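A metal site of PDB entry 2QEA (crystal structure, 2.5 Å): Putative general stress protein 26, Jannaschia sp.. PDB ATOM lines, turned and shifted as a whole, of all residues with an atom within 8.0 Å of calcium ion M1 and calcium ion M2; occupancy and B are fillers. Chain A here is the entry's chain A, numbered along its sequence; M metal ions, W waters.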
ATOM      1  N   HIS A   7     -18.261 -21.328  11.062  1.00  0.00           N
ATOM      2  CA  HIS A   7     -18.824 -22.185   9.997  1.00  0.00           C
ATOM      3  C   HIS A   7     -17.877 -22.297   8.798  1.00  0.00           C
ATOM      4  O   HIS A   7     -17.692 -23.389   8.272  1.00  0.00           O
ATOM      5  CB  HIS A   7     -20.205 -21.687   9.519  1.00  0.00           C
ATOM      6  CG  HIS A   7     -21.318 -21.937  10.478  1.00  0.00           C
ATOM      7  ND1 HIS A   7     -21.924 -20.934  11.214  1.00  0.00           N
ATOM      8  CD2 HIS A   7     -21.951 -23.086  10.830  1.00  0.00           C
ATOM      9  CE1 HIS A   7     -22.873 -21.445  11.972  1.00  0.00           C
ATOM     10  NE2 HIS A   7     -22.909 -22.748  11.757  1.00  0.00           N
ATOM     11  N   GLU A   8     -17.268 -21.172   8.411  1.00  0.00           N
ATOM     12  CA  GLU A   8     -16.307 -21.129   7.295  1.00  0.00           C
ATOM     13  C   GLU A   8     -14.995 -21.882   7.592  1.00  0.00           C
ATOM     14  O   GLU A   8     -14.363 -22.389   6.658  1.00  0.00           O
ATOM     15  CB  GLU A   8     -16.015 -19.666   6.899  1.00  0.00           C
ATOM     16  CG  GLU A   8     -15.237 -19.461   5.585  1.00  0.00           C
ATOM     17  CD  GLU A   8     -15.984 -19.923   4.333  1.00  0.00           C
ATOM     18  OE1 GLU A   8     -17.189 -20.240   4.396  1.00  0.00           O
ATOM     19  OE2 GLU A   8     -15.363 -19.959   3.259  1.00  0.00           O
ATOM     20  N   PHE A   9     -14.592 -21.925   8.864  1.00  0.00           N
ATOM     21  CA  PHE A   9     -13.418 -22.696   9.289  1.00  0.00           C
ATOM     22  C   PHE A   9     -13.639 -24.189   8.982  1.00  0.00           C
ATOM     23  O   PHE A   9     -12.804 -24.824   8.332  1.00  0.00           O
ATOM     24  CB  PHE A   9     -13.075 -22.472  10.784  1.00  0.00           C
ATOM     25  CG  PHE A   9     -12.143 -23.498  11.373  1.00  0.00           C
ATOM     26  CD1 PHE A   9     -10.769 -23.370  11.237  1.00  0.00           C
ATOM     27  CD2 PHE A   9     -12.661 -24.606  12.048  1.00  0.00           C
ATOM     28  CE1 PHE A   9      -9.906 -24.337  11.775  1.00  0.00           C
ATOM     29  CE2 PHE A   9     -11.815 -25.585  12.590  1.00  0.00           C
ATOM     30  CZ  PHE A   9     -10.432 -25.445  12.462  1.00  0.00           C
ATOM     31  N   TRP A  10     -14.769 -24.732   9.448  1.00  0.00           N
ATOM     32  CA  TRP A  10     -15.144 -26.145   9.206  1.00  0.00           C
ATOM     33  C   TRP A  10     -15.398 -26.407   7.717  1.00  0.00           C
ATOM     34  O   TRP A  10     -15.143 -27.509   7.229  1.00  0.00           O
ATOM     35  CB  TRP A  10     -16.387 -26.558  10.001  1.00  0.00           C
ATOM     36  CG  TRP A  10     -16.194 -26.528  11.480  1.00  0.00           C
ATOM     37  CD1 TRP A  10     -16.747 -25.645  12.354  1.00  0.00           C
ATOM     38  CD2 TRP A  10     -15.363 -27.395  12.253  1.00  0.00           C
ATOM     39  NE1 TRP A  10     -16.342 -25.910  13.635  1.00  0.00           N
ATOM     40  CE2 TRP A  10     -15.483 -26.987  13.609  1.00  0.00           C
ATOM     41  CE3 TRP A  10     -14.534 -28.480  11.948  1.00  0.00           C
ATOM     42  CZ2 TRP A  10     -14.800 -27.630  14.653  1.00  0.00           C
ATOM     43  CZ3 TRP A  10     -13.849 -29.132  12.992  1.00  0.00           C
ATOM     44  CH2 TRP A  10     -13.999 -28.690  14.321  1.00  0.00           C
ATOM     45  N   ASP A  11     -15.927 -25.393   7.026  1.00  0.00           N
ATOM     46  CA  ASP A  11     -16.201 -25.445   5.593  1.00  0.00           C
ATOM     47  C   ASP A  11     -14.908 -25.711   4.817  1.00  0.00           C
ATOM     48  O   ASP A  11     -14.879 -26.609   3.985  1.00  0.00           O
ATOM     49  CB  ASP A  11     -16.853 -24.122   5.146  1.00  0.00           C
ATOM     50  CG  ASP A  11     -17.420 -24.166   3.744  1.00  0.00           C
ATOM     51  OD1 ASP A  11     -17.376 -25.201   3.057  1.00  0.00           O
ATOM     52  OD2 ASP A  11     -17.957 -23.129   3.308  1.00  0.00           O
ATOM     53  N   ARG A  12     -13.856 -24.946   5.108  1.00  0.00           N
ATOM     54  CA  ARG A  12     -12.571 -25.072   4.399  1.00  0.00           C
ATOM     55  C   ARG A  12     -11.604 -26.135   4.923  1.00  0.00           C
ATOM     56  O   ARG A  12     -10.772 -26.610   4.155  1.00  0.00           O
ATOM     57  CB  ARG A  12     -11.883 -23.718   4.344  1.00  0.00           C
ATOM     58  CG  ARG A  12     -12.683 -22.695   3.580  1.00  0.00           C
ATOM     59  CD  ARG A  12     -11.938 -21.414   3.497  1.00  0.00           C
ATOM     60  NE  ARG A  12     -12.683 -20.392   2.754  1.00  0.00           N
ATOM     61  CZ  ARG A  12     -12.267 -19.141   2.588  1.00  0.00           C
ATOM     62  NH1 ARG A  12     -11.089 -18.728   3.065  1.00  0.00           N
ATOM     63  NH2 ARG A  12     -13.036 -18.283   1.917  1.00  0.00           N
ATOM     64  N   LEU A  13     -11.717 -26.506   6.208  1.00  0.00           N
ATOM     65  CA  LEU A  13     -10.823 -27.498   6.833  1.00  0.00           C
ATOM     66  C   LEU A  13     -10.808 -28.890   6.155  1.00  0.00           C
ATOM     67  O   LEU A  13      -9.802 -29.591   6.220  1.00  0.00           O
ATOM     68  CB  LEU A  13     -11.113 -27.639   8.343  1.00  0.00           C
ATOM     69  CG  LEU A  13     -10.219 -28.546   9.208  1.00  0.00           C
ATOM     70  CD1 LEU A  13      -8.757 -28.171   9.077  1.00  0.00           C
ATOM     71  CD2 LEU A  13     -10.663 -28.478  10.655  1.00  0.00           C
ATOM     72  N   GLU A  14     -11.910 -29.254   5.511  1.00  0.00           N
ATOM     73  CA  GLU A  14     -12.037 -30.527   4.762  1.00  0.00           C
ATOM     74  C   GLU A  14     -10.993 -30.694   3.660  1.00  0.00           C
ATOM     75  O   GLU A  14     -10.415 -31.774   3.501  1.00  0.00           O
ATOM     76  CB  GLU A  14     -13.395 -30.605   4.070  1.00  0.00           C
ATOM     77  CG  GLU A  14     -14.563 -30.733   4.992  1.00  0.00           C
ATOM     78  CD  GLU A  14     -15.850 -30.741   4.234  1.00  0.00           C
ATOM     79  OE1 GLU A  14     -16.099 -29.799   3.447  1.00  0.00           O
ATOM     80  OE2 GLU A  14     -16.645 -31.694   4.413  1.00  0.00           O
ATOM     81  N   ASP A  15     -10.794 -29.625   2.890  1.00  0.00           N
ATOM     82  CA  ASP A  15      -9.808 -29.598   1.790  1.00  0.00           C
ATOM     83  C   ASP A  15      -8.341 -29.386   2.234  1.00  0.00           C
ATOM     84  O   ASP A  15      -7.441 -29.418   1.396  1.00  0.00           O
ATOM     85  CB  ASP A  15     -10.203 -28.539   0.739  1.00  0.00           C
ATOM     86  CG  ASP A  15     -11.489 -28.891  -0.005  1.00  0.00           C
ATOM     87  OD1 ASP A  15     -12.307 -29.701   0.498  1.00  0.00           O
ATOM     88  OD2 ASP A  15     -11.697 -28.332  -1.099  1.00  0.00           O
ATOM     89  N   THR A  36     -12.060 -34.500   8.313  1.00  0.00           N
ATOM     90  CA  THR A  36     -13.312 -33.888   8.803  1.00  0.00           C
ATOM     91  C   THR A  36     -14.426 -33.956   7.763  1.00  0.00           C
ATOM     92  O   THR A  36     -14.188 -34.302   6.597  1.00  0.00           O
ATOM     93  CB  THR A  36     -13.111 -32.407   9.216  1.00  0.00           C
ATOM     94  OG1 THR A  36     -12.745 -31.622   8.072  1.00  0.00           O
ATOM     95  CG2 THR A  36     -12.025 -32.262  10.278  1.00  0.00           C
ATOM     96  N   ASP A  37     -15.629 -33.651   8.217  1.00  0.00           N
ATOM     97  CA  ASP A  37     -16.827 -33.596   7.379  1.00  0.00           C
ATOM     98  C   ASP A  37     -17.639 -32.414   7.911  1.00  0.00           C
ATOM     99  O   ASP A  37     -18.023 -32.412   9.076  1.00  0.00           O
ATOM    100  CB  ASP A  37     -17.606 -34.912   7.469  1.00  0.00           C
ATOM    101  CG  ASP A  37     -18.666 -35.074   6.371  1.00  0.00           C
ATOM    102  OD1 ASP A  37     -19.194 -34.068   5.844  1.00  0.00           O
ATOM    103  OD2 ASP A  37     -18.978 -36.237   6.047  1.00  0.00           O
ATOM    104  N   ASP A  38     -17.908 -31.415   7.053  1.00  0.00           N
ATOM    105  CA  ASP A  38     -18.667 -30.206   7.453  1.00  0.00           C
ATOM    106  C   ASP A  38     -20.167 -30.443   7.707  1.00  0.00           C
ATOM    107  O   ASP A  38     -20.854 -29.526   8.156  1.00  0.00           O
ATOM    108  CB  ASP A  38     -18.391 -28.976   6.561  1.00  0.00           C
ATOM    109  CG  ASP A  38     -18.775 -29.166   5.092  1.00  0.00           C
ATOM    110  OD1 ASP A  38     -19.278 -30.236   4.696  1.00  0.00           O
ATOM    111  OD2 ASP A  38     -18.537 -28.213   4.330  1.00  0.00           O
ATOM    112  N   ASP A  39     -20.671 -31.643   7.377  1.00  0.00           N
ATOM    113  CA  ASP A  39     -22.029 -32.070   7.756  1.00  0.00           C
ATOM    114  C   ASP A  39     -22.084 -32.338   9.271  1.00  0.00           C
ATOM    115  O   ASP A  39     -23.106 -32.064   9.907  1.00  0.00           O
ATOM    116  CB  ASP A  39     -22.471 -33.319   6.991  1.00  0.00           C
ATOM    117  CG  ASP A  39     -22.635 -33.082   5.486  1.00  0.00           C
ATOM    118  OD1 ASP A  39     -22.236 -32.011   4.975  1.00  0.00           O
ATOM    119  OD2 ASP A  39     -23.161 -33.989   4.813  1.00  0.00           O
ATOM    120  N   GLU A  74      -6.506 -23.032   0.197  1.00  0.00           N
ATOM    121  CA  GLU A  74      -7.809 -22.759   0.812  1.00  0.00           C
ATOM    122  C   GLU A  74      -7.899 -21.397   1.504  1.00  0.00           C
ATOM    123  O   GLU A  74      -8.995 -20.888   1.697  1.00  0.00           O
ATOM    124  CB  GLU A  74      -8.173 -23.879   1.816  1.00  0.00           C
ATOM    125  CG  GLU A  74      -8.384 -25.244   1.158  1.00  0.00           C
ATOM    126  CD  GLU A  74      -9.567 -25.240   0.187  1.00  0.00           C
ATOM    127  OE1 GLU A  74     -10.680 -24.841   0.591  1.00  0.00           O
ATOM    128  OE2 GLU A  74      -9.379 -25.665  -0.977  1.00  0.00           O
HETATM  129 CA    CA M   1     -16.615 -27.582   2.644  1.00  0.00          CA
HETATM  130 CA    CA M   2     -18.317 -31.495   2.383  1.00  0.00          CA
HETATM  131  O   HOH W   1     -15.038 -28.362   0.599  1.00  0.00           O
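Three residues have an atom within 4 Å of calcium ion M1: Asp 11, Glu 14 and Asp 38.
The nearest printed residue that does not touch calcium ion M1 is Arg 12 (4.5 Å).
The nearest printed residue that does not touch calcium ion M2 is Asp 37 (4.4 Å).
Calcium ion M1 is bound by O of Asp 11 (2.4 Å).
Calcium ion M1 is bound by the side-chain carboxylate (OE1) of Glu 14, at 2.4 Å.
OD1 of Asp 11 binds calcium ion M1 (2.5 Å).
Calcium ion M1 is bound by OD2 of Asp 38 (2.6 Å).
Calcium ion M1 is bound by water W1 (2.7 Å).
OE2 of Glu 14 is bound to calcium ion M2, 2.6 Å away.
OD1 of Asp 38 binds calcium ion M2 (2.8 Å).
Calcium ion M2 has two donor atoms within binding distance.
Slightly farther from calcium ion M2 lies the side-chain carboxylate (OE1) of Glu 14 (3.0 Å).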
